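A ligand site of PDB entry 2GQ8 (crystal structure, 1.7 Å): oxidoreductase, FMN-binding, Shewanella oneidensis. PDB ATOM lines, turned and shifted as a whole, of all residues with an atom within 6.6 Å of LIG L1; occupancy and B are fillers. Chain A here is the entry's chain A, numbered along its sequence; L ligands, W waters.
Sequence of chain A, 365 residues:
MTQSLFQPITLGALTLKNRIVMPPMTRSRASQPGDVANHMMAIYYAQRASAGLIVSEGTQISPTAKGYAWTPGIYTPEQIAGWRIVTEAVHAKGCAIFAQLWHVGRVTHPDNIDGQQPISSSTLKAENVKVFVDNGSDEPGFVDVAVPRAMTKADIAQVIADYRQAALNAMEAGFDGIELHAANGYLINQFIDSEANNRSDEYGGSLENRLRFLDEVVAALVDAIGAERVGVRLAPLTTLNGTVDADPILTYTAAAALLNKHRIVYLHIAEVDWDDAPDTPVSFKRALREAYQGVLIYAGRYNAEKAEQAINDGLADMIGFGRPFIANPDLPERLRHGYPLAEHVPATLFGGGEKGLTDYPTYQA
ND2 of Asn 184 lies within hydrogen-bond range of O1 of LIG L1 (2.6 Å). A ring nitrogen (NE2) of His 181 sits at hydrogen-bond distance from an oxygen (O1) of LIG L1, 2.7 Å away. NE2 of His 181 is in hydrogen-bond range of O1 of LG2 L2. N of Thr 26 is in hydrogen-bond range of N3 of LG2 L2 (2.8 Å). O2 of LG2 L2 sits at hydrogen-bond distance from OG1 of Thr 26 (2.7 Å). The guanidinium group (NH2) of Arg 233 sits at hydrogen-bond distance from an oxygen (O4) of LG2 L2, 2.8 Å away. The side-chain amide nitrogen (NE2) of Gln 100 sits at hydrogen-bond distance from an oxygen (O1) of LG2 L2 (2.8 Å). O of Pro 24 is in hydrogen-bond range of O3 of LG2 L2, at 2.7 Å. An oxygen (O2) of LG2 L2 is in hydrogen-bond range of the backbone NH of Gly 58 (3.1 Å).
Water W2 lies within hydrogen-bond range of OD1 of Asp 273 and ND2 of Asn 241. Water W1 bridges the side-chain carboxylate of Asp 273 (2.7 Å) and the indole nitrogen of Trp 274 (2.9 Å).
A nitrogen (N1) of LG2 L2 lies close to an oxygen (O1) of LIG L1 (3.1 Å).
Residues that only touch LIG L1: Thr 26 (3.7 Å), Tyr 68 (3.8 Å), Trp 102 (3.4 Å), Tyr 186 (3.3 Å), Asp 273 (3.7 Å), Trp 274 (3.3 Å) and Phe 350 (3.6 Å). Hydrophobic or aromatic side chains within 4 Å of LIG L1: Tyr 68, Trp 102, His 181, Tyr 186, Trp 274 and Phe 350.
The backbone carbonyl oxygen (O) of Asn 184 lies within hydrogen-bond range of the side-chain amide nitrogen (ND2) of Asn 241, at 2.8 Å. ND1 of His 181 lies within hydrogen-bond range of N of Ala 183 (3.1 Å). The side-chain hydroxyl of Tyr 186 lies within hydrogen-bond range of the side-chain hydroxyl of Tyr 68 (2.7 Å). ND2 of Asn 241 sits at hydrogen-bond distance from OH of Tyr 186 (3.3 Å). The backbone carbonyl oxygen (O) of Tyr 68 is in hydrogen-bond range of the side-chain hydroxyl (OG1) of Thr 71 (3.5 Å).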
ATOM      1  N   PRO A  24      14.795 -24.975  12.072  1.00  0.00           N
ATOM      2  CA  PRO A  24      15.698 -25.089  13.216  1.00  0.00           C
ATOM      3  C   PRO A  24      16.950 -24.244  13.011  1.00  0.00           C
ATOM      4  O   PRO A  24      17.593 -24.355  11.969  1.00  0.00           O
ATOM      5  CB  PRO A  24      16.002 -26.592  13.271  1.00  0.00           C
ATOM      6  CG  PRO A  24      15.877 -27.016  11.849  1.00  0.00           C
ATOM      7  CD  PRO A  24      14.652 -26.269  11.382  1.00  0.00           C
ATOM      8  N   MET A  25      17.276 -23.399  13.985  1.00  0.00           N
ATOM      9  CA  MET A  25      18.462 -22.566  13.876  1.00  0.00           C
ATOM     10  C   MET A  25      19.199 -22.397  15.191  1.00  0.00           C
ATOM     11  O   MET A  25      18.733 -21.724  16.106  1.00  0.00           O
ATOM     12  CB  MET A  25      18.124 -21.190  13.291  1.00  0.00           C
ATOM     13  CG  MET A  25      17.727 -21.266  11.828  1.00  0.00           C
ATOM     14  SD  MET A  25      17.358 -19.649  11.111  1.00  0.00           S
ATOM     15  CE  MET A  25      15.822 -19.228  11.998  1.00  0.00           C
ATOM     16  N   THR A  26      20.348 -23.057  15.277  1.00  0.00           N
ATOM     17  CA  THR A  26      21.208 -22.988  16.441  1.00  0.00           C
ATOM     18  C   THR A  26      21.615 -21.540  16.693  1.00  0.00           C
ATOM     19  O   THR A  26      22.106 -20.882  15.788  1.00  0.00           O
ATOM     20  CB  THR A  26      22.490 -23.803  16.191  1.00  0.00           C
ATOM     21  OG1 THR A  26      22.162 -25.183  16.105  1.00  0.00           O
ATOM     22  CG2 THR A  26      23.503 -23.593  17.327  1.00  0.00           C
ATOM     23  N   SER A  28      23.017 -20.872  19.985  1.00  0.00           N
ATOM     24  CA  SER A  28      23.958 -21.029  21.084  1.00  0.00           C
ATOM     25  C   SER A  28      23.815 -19.975  22.176  1.00  0.00           C
ATOM     26  O   SER A  28      24.781 -19.284  22.542  1.00  0.00           O
ATOM     27  CB  SER A  28      25.388 -21.031  20.546  1.00  0.00           C
ATOM     28  OG  SER A  28      25.594 -22.183  19.728  1.00  0.00           O
ATOM     29  N   GLY A  58      18.580 -27.153  16.982  1.00  0.00           N
ATOM     30  CA  GLY A  58      18.963 -28.488  17.400  1.00  0.00           C
ATOM     31  C   GLY A  58      19.172 -28.536  18.903  1.00  0.00           C
ATOM     32  O   GLY A  58      19.767 -27.630  19.487  1.00  0.00           O
ATOM     33  N   TYR A  68      28.420 -28.017  19.294  1.00  0.00           N
ATOM     34  CA  TYR A  68      28.769 -26.602  19.384  1.00  0.00           C
ATOM     35  C   TYR A  68      28.538 -26.067  20.783  1.00  0.00           C
ATOM     36  O   TYR A  68      27.646 -26.513  21.503  1.00  0.00           O
ATOM     37  CB  TYR A  68      27.939 -25.791  18.391  1.00  0.00           C
ATOM     38  CG  TYR A  68      28.002 -26.335  16.985  1.00  0.00           C
ATOM     39  CD1 TYR A  68      28.895 -25.796  16.051  1.00  0.00           C
ATOM     40  CD2 TYR A  68      27.230 -27.416  16.614  1.00  0.00           C
ATOM     41  CE1 TYR A  68      29.000 -26.344  14.770  1.00  0.00           C
ATOM     42  CE2 TYR A  68      27.323 -27.982  15.354  1.00  0.00           C
ATOM     43  CZ  TYR A  68      28.210 -27.445  14.443  1.00  0.00           C
ATOM     44  OH  TYR A  68      28.303 -28.035  13.205  1.00  0.00           O
ATOM     45  N   THR A  71      24.742 -24.854  23.121  1.00  0.00           N
ATOM     46  CA  THR A  71      23.474 -25.265  22.534  1.00  0.00           C
ATOM     47  C   THR A  71      22.666 -25.912  23.658  1.00  0.00           C
ATOM     48  O   THR A  71      23.210 -26.571  24.540  1.00  0.00           O
ATOM     49  CB  THR A  71      23.667 -26.255  21.342  1.00  0.00           C
ATOM     50  OG1 THR A  71      24.327 -27.450  21.779  1.00  0.00           O
ATOM     51  CG2 THR A  71      24.513 -25.582  20.239  1.00  0.00           C
ATOM     52  N   GLN A 100      13.856 -30.096  17.703  1.00  0.00           N
ATOM     53  CA  GLN A 100      14.718 -30.849  16.794  1.00  0.00           C
ATOM     54  C   GLN A 100      15.718 -31.647  17.612  1.00  0.00           C
ATOM     55  O   GLN A 100      16.680 -31.087  18.168  1.00  0.00           O
ATOM     56  CB  GLN A 100      15.481 -29.947  15.810  1.00  0.00           C
ATOM     57  CG  GLN A 100      16.296 -30.797  14.816  1.00  0.00           C
ATOM     58  CD  GLN A 100      17.199 -30.003  13.909  1.00  0.00           C
ATOM     59  OE1 GLN A 100      18.115 -29.310  14.364  1.00  0.00           O
ATOM     60  NE2 GLN A 100      16.955 -30.119  12.601  1.00  0.00           N
ATOM     61  N   TRP A 102      18.771 -33.682  18.348  1.00  0.00           N
ATOM     62  CA  TRP A 102      20.082 -33.657  17.718  1.00  0.00           C
ATOM     63  C   TRP A 102      21.192 -34.544  18.255  1.00  0.00           C
ATOM     64  O   TRP A 102      21.394 -34.649  19.463  1.00  0.00           O
ATOM     65  CB  TRP A 102      20.554 -32.200  17.798  1.00  0.00           C
ATOM     66  CG  TRP A 102      21.594 -31.733  16.843  1.00  0.00           C
ATOM     67  CD1 TRP A 102      21.994 -32.323  15.673  1.00  0.00           C
ATOM     68  CD2 TRP A 102      22.273 -30.474  16.911  1.00  0.00           C
ATOM     69  NE1 TRP A 102      22.873 -31.499  15.009  1.00  0.00           N
ATOM     70  CE2 TRP A 102      23.071 -30.362  15.744  1.00  0.00           C
ATOM     71  CE3 TRP A 102      22.297 -29.422  17.847  1.00  0.00           C
ATOM     72  CZ2 TRP A 102      23.867 -29.234  15.487  1.00  0.00           C
ATOM     73  CZ3 TRP A 102      23.077 -28.308  17.596  1.00  0.00           C
ATOM     74  CH2 TRP A 102      23.859 -28.220  16.419  1.00  0.00           C
ATOM     75  N   PHE A 132      32.604 -24.855  16.983  1.00  0.00           N
ATOM     76  CA  PHE A 132      33.156 -23.880  17.901  1.00  0.00           C
ATOM     77  C   PHE A 132      32.970 -24.328  19.339  1.00  0.00           C
ATOM     78  O   PHE A 132      32.012 -25.034  19.663  1.00  0.00           O
ATOM     79  CB  PHE A 132      32.586 -22.469  17.658  1.00  0.00           C
ATOM     80  CG  PHE A 132      31.080 -22.375  17.758  1.00  0.00           C
ATOM     81  CD1 PHE A 132      30.436 -22.328  19.001  1.00  0.00           C
ATOM     82  CD2 PHE A 132      30.303 -22.264  16.604  1.00  0.00           C
ATOM     83  CE1 PHE A 132      29.053 -22.164  19.076  1.00  0.00           C
ATOM     84  CE2 PHE A 132      28.923 -22.113  16.674  1.00  0.00           C
ATOM     85  CZ  PHE A 132      28.298 -22.060  17.915  1.00  0.00           C
ATOM     86  N   HIS A 181      16.788 -34.729  13.511  1.00  0.00           N
ATOM     87  CA  HIS A 181      17.791 -34.144  12.631  1.00  0.00           C
ATOM     88  C   HIS A 181      18.590 -35.296  12.014  1.00  0.00           C
ATOM     89  O   HIS A 181      19.448 -35.887  12.672  1.00  0.00           O
ATOM     90  CB  HIS A 181      18.748 -33.248  13.409  1.00  0.00           C
ATOM     91  CG  HIS A 181      19.543 -32.324  12.538  1.00  0.00           C
ATOM     92  ND1 HIS A 181      19.672 -32.512  11.176  1.00  0.00           N
ATOM     93  CD2 HIS A 181      20.209 -31.180  12.832  1.00  0.00           C
ATOM     94  CE1 HIS A 181      20.399 -31.527  10.665  1.00  0.00           C
ATOM     95  NE2 HIS A 181      20.735 -30.708  11.651  1.00  0.00           N
ATOM     96  N   ALA A 183      19.887 -34.740   8.974  1.00  0.00           N
ATOM     97  CA  ALA A 183      20.467 -33.990   7.877  1.00  0.00           C
ATOM     98  C   ALA A 183      21.797 -33.323   8.222  1.00  0.00           C
ATOM     99  O   ALA A 183      22.442 -33.630   9.228  1.00  0.00           O
ATOM    100  CB  ALA A 183      19.457 -32.911   7.410  1.00  0.00           C
ATOM    101  N   ASN A 184      22.184 -32.430   7.321  1.00  0.00           N
ATOM    102  CA  ASN A 184      23.384 -31.615   7.400  1.00  0.00           C
ATOM    103  C   ASN A 184      24.665 -32.224   7.954  1.00  0.00           C
ATOM    104  O   ASN A 184      25.415 -31.577   8.680  1.00  0.00           O
ATOM    105  CB  ASN A 184      23.046 -30.319   8.135  1.00  0.00           C
ATOM    106  CG  ASN A 184      21.914 -29.577   7.446  1.00  0.00           C
ATOM    107  OD1 ASN A 184      21.656 -29.793   6.256  1.00  0.00           O
ATOM    108  ND2 ASN A 184      21.239 -28.702   8.170  1.00  0.00           N
ATOM    109  N   GLY A 185      24.894 -33.471   7.565  1.00  0.00           N
ATOM    110  CA  GLY A 185      26.102 -34.174   7.943  1.00  0.00           C
ATOM    111  C   GLY A 185      26.239 -34.645   9.369  1.00  0.00           C
ATOM    112  O   GLY A 185      27.330 -35.016   9.791  1.00  0.00           O
ATOM    113  N   TYR A 186      25.150 -34.642  10.119  1.00  0.00           N
ATOM    114  CA  TYR A 186      25.251 -35.090  11.500  1.00  0.00           C
ATOM    115  C   TYR A 186      25.173 -36.609  11.653  1.00  0.00           C
ATOM    116  O   TYR A 186      25.270 -37.323  10.658  1.00  0.00           O
ATOM    117  CB  TYR A 186      24.278 -34.309  12.361  1.00  0.00           C
ATOM    118  CG  TYR A 186      24.686 -32.851  12.374  1.00  0.00           C
ATOM    119  CD1 TYR A 186      23.907 -31.876  11.758  1.00  0.00           C
ATOM    120  CD2 TYR A 186      25.909 -32.449  12.931  1.00  0.00           C
ATOM    121  CE1 TYR A 186      24.341 -30.553  11.670  1.00  0.00           C
ATOM    122  CE2 TYR A 186      26.347 -31.126  12.866  1.00  0.00           C
ATOM    123  CZ  TYR A 186      25.552 -30.179  12.231  1.00  0.00           C
ATOM    124  OH  TYR A 186      25.990 -28.878  12.121  1.00  0.00           O
ATOM    125  N   ARG A 233      14.173 -34.550   9.287  1.00  0.00           N
ATOM    126  CA  ARG A 233      14.860 -33.649   8.359  1.00  0.00           C
ATOM    127  C   ARG A 233      15.985 -34.376   7.628  1.00  0.00           C
ATOM    128  O   ARG A 233      16.772 -35.092   8.259  1.00  0.00           O
ATOM    129  CB  ARG A 233      15.443 -32.426   9.085  1.00  0.00           C
ATOM    130  CG  ARG A 233      15.823 -31.314   8.107  1.00  0.00           C
ATOM    131  CD  ARG A 233      16.222 -30.002   8.776  1.00  0.00           C
ATOM    132  NE  ARG A 233      15.803 -28.857   7.962  1.00  0.00           N
ATOM    133  CZ  ARG A 233      16.404 -27.667   7.930  1.00  0.00           C
ATOM    134  NH1 ARG A 233      17.481 -27.425   8.659  1.00  0.00           N
ATOM    135  NH2 ARG A 233      15.902 -26.707   7.165  1.00  0.00           N
ATOM    136  N   ASN A 241      29.016 -30.263   5.557  1.00  0.00           N
ATOM    137  CA  ASN A 241      29.640 -30.861   6.733  1.00  0.00           C
ATOM    138  C   ASN A 241      30.379 -32.174   6.500  1.00  0.00           C
ATOM    139  O   ASN A 241      30.677 -32.899   7.439  1.00  0.00           O
ATOM    140  CB  ASN A 241      28.627 -31.009   7.874  1.00  0.00           C
ATOM    141  CG  ASN A 241      28.460 -29.723   8.669  1.00  0.00           C
ATOM    142  OD1 ASN A 241      29.424 -28.978   8.862  1.00  0.00           O
ATOM    143  ND2 ASN A 241      27.246 -29.463   9.132  1.00  0.00           N
ATOM    144  N   ASP A 273      22.487 -25.221   2.696  1.00  0.00           N
ATOM    145  CA  ASP A 273      23.114 -25.142   4.012  1.00  0.00           C
ATOM    146  C   ASP A 273      24.139 -24.030   3.829  1.00  0.00           C
ATOM    147  O   ASP A 273      25.136 -24.217   3.138  1.00  0.00           O
ATOM    148  CB  ASP A 273      23.801 -26.445   4.402  1.00  0.00           C
ATOM    149  CG  ASP A 273      24.007 -26.559   5.894  1.00  0.00           C
ATOM    150  OD1 ASP A 273      24.941 -27.277   6.313  1.00  0.00           O
ATOM    151  OD2 ASP A 273      23.237 -25.934   6.666  1.00  0.00           O
ATOM    152  N   TRP A 274      23.865 -22.871   4.431  1.00  0.00           N
ATOM    153  CA  TRP A 274      24.731 -21.696   4.306  1.00  0.00           C
ATOM    154  C   TRP A 274      24.854 -21.299   2.839  1.00  0.00           C
ATOM    155  O   TRP A 274      23.874 -20.826   2.252  1.00  0.00           O
ATOM    156  CB  TRP A 274      26.110 -21.973   4.927  1.00  0.00           C
ATOM    157  CG  TRP A 274      26.014 -22.174   6.408  1.00  0.00           C
ATOM    158  CD1 TRP A 274      26.135 -23.347   7.091  1.00  0.00           C
ATOM    159  CD2 TRP A 274      25.741 -21.167   7.389  1.00  0.00           C
ATOM    160  NE1 TRP A 274      25.951 -23.129   8.438  1.00  0.00           N
ATOM    161  CE2 TRP A 274      25.711 -21.798   8.650  1.00  0.00           C
ATOM    162  CE3 TRP A 274      25.523 -19.778   7.324  1.00  0.00           C
ATOM    163  CZ2 TRP A 274      25.461 -21.102   9.844  1.00  0.00           C
ATOM    164  CZ3 TRP A 274      25.283 -19.083   8.508  1.00  0.00           C
ATOM    165  CH2 TRP A 274      25.250 -19.752   9.744  1.00  0.00           C
ATOM    166  N   PHE A 350      25.650 -16.625  16.813  1.00  0.00           N
ATOM    167  CA  PHE A 350      25.980 -17.550  17.897  1.00  0.00           C
ATOM    168  C   PHE A 350      26.544 -16.923  19.149  1.00  0.00           C
ATOM    169  O   PHE A 350      27.414 -16.033  19.090  1.00  0.00           O
ATOM    170  CB  PHE A 350      26.981 -18.605  17.411  1.00  0.00           C
ATOM    171  CG  PHE A 350      26.597 -19.251  16.124  1.00  0.00           C
ATOM    172  CD1 PHE A 350      27.318 -18.990  14.960  1.00  0.00           C
ATOM    173  CD2 PHE A 350      25.524 -20.125  16.063  1.00  0.00           C
ATOM    174  CE1 PHE A 350      26.972 -19.583  13.748  1.00  0.00           C
ATOM    175  CE2 PHE A 350      25.163 -20.733  14.858  1.00  0.00           C
ATOM    176  CZ  PHE A 350      25.889 -20.456  13.698  1.00  0.00           C
HETATM  177  C1  LIG L   1      22.743 -27.617  11.317  1.00  0.00           C
HETATM  178  C2  LIG L   1      23.203 -26.554  10.275  1.00  0.00           C
HETATM  179  C3  LIG L   1      23.933 -25.527  10.875  1.00  0.00           C
HETATM  180  C4  LIG L   1      24.314 -25.454  12.228  1.00  0.00           C
HETATM  181  C5  LIG L   1      23.814 -26.447  13.089  1.00  0.00           C
HETATM  182  C6  LIG L   1      23.026 -27.527  12.684  1.00  0.00           C
HETATM  183  O1  LIG L   1      21.952 -28.517  10.709  1.00  0.00           O
HETATM  184  O2  LIG L   1      25.681 -23.585  11.942  1.00  0.00           O
HETATM  185  C7  LIG L   1      25.212 -24.545  12.865  1.00  0.00           C
HETATM  186  C8  LIG L   1      25.858 -24.322  14.242  1.00  0.00           C
HETATM  187  N1  LG2 L   2      19.507 -26.599  10.446  1.00  0.00           N
HETATM  188  C1  LG2 L   2      19.110 -27.649  11.303  1.00  0.00           C
HETATM  189  O1  LG2 L   2      18.589 -28.638  10.897  1.00  0.00           O
HETATM  190  N2  LG2 L   2      19.449 -27.533  12.679  1.00  0.00           N
HETATM  191  C2  LG2 L   2      19.788 -26.373  13.280  1.00  0.00           C
HETATM  192  O2  LG2 L   2      20.283 -26.320  14.575  1.00  0.00           O
HETATM  193  C3  LG2 L   2      20.401 -25.276  12.399  1.00  0.00           C
HETATM  194  N3  LG2 L   2      21.171 -24.244  12.862  1.00  0.00           N
HETATM  195  C4  LG2 L   2      21.325 -23.180  12.032  1.00  0.00           C
HETATM  196  C5  LG2 L   2      21.993 -21.963  12.682  1.00  0.00           C
HETATM  197  C6  LG2 L   2      22.102 -20.787  11.851  1.00  0.00           C
HETATM  198  C7  LG2 L   2      22.460 -19.493  12.563  1.00  0.00           C
HETATM  199  C8  LG2 L   2      21.511 -20.668  10.547  1.00  0.00           C
HETATM  200  C9  LG2 L   2      21.502 -19.534   9.491  1.00  0.00           C
HETATM  201  C10 LG2 L   2      21.029 -21.838   9.896  1.00  0.00           C
HETATM  202  C11 LG2 L   2      20.943 -23.182  10.610  1.00  0.00           C
HETATM  203  N4  LG2 L   2      20.283 -24.391  10.158  1.00  0.00           N
HETATM  204  C12 LG2 L   2      19.992 -25.473  10.963  1.00  0.00           C
HETATM  205  C13 LG2 L   2      19.861 -24.495   8.753  1.00  0.00           C
HETATM  206  C14 LG2 L   2      18.496 -23.816   8.613  1.00  0.00           C
HETATM  207  O3  LG2 L   2      17.454 -24.526   9.276  1.00  0.00           O
HETATM  208  C15 LG2 L   2      18.121 -23.632   7.130  1.00  0.00           C
HETATM  209  O4  LG2 L   2      17.919 -24.936   6.513  1.00  0.00           O
HETATM  210  C16 LG2 L   2      19.094 -22.823   6.294  1.00  0.00           C
HETATM  211  O5  LG2 L   2      19.449 -21.599   6.985  1.00  0.00           O
HETATM  212  C17 LG2 L   2      18.665 -22.530   4.880  1.00  0.00           C
HETATM  213  O6  LG2 L   2      17.508 -21.673   4.861  1.00  0.00           O
HETATM  214  P1  LG2 L   2      17.638 -20.099   4.613  1.00  0.00           P
HETATM  215  O7  LG2 L   2      18.332 -19.487   5.783  1.00  0.00           O
HETATM  216  O8  LG2 L   2      18.362 -19.886   3.306  1.00  0.00           O
HETATM  217  O9  LG2 L   2      16.156 -19.648   4.487  1.00  0.00           O
HETATM  218  O   HOH W   1      23.117 -23.634   8.068  1.00  0.00           O
HETATM  219  O   HOH W   2      26.032 -26.718   8.831  1.00  0.00           O
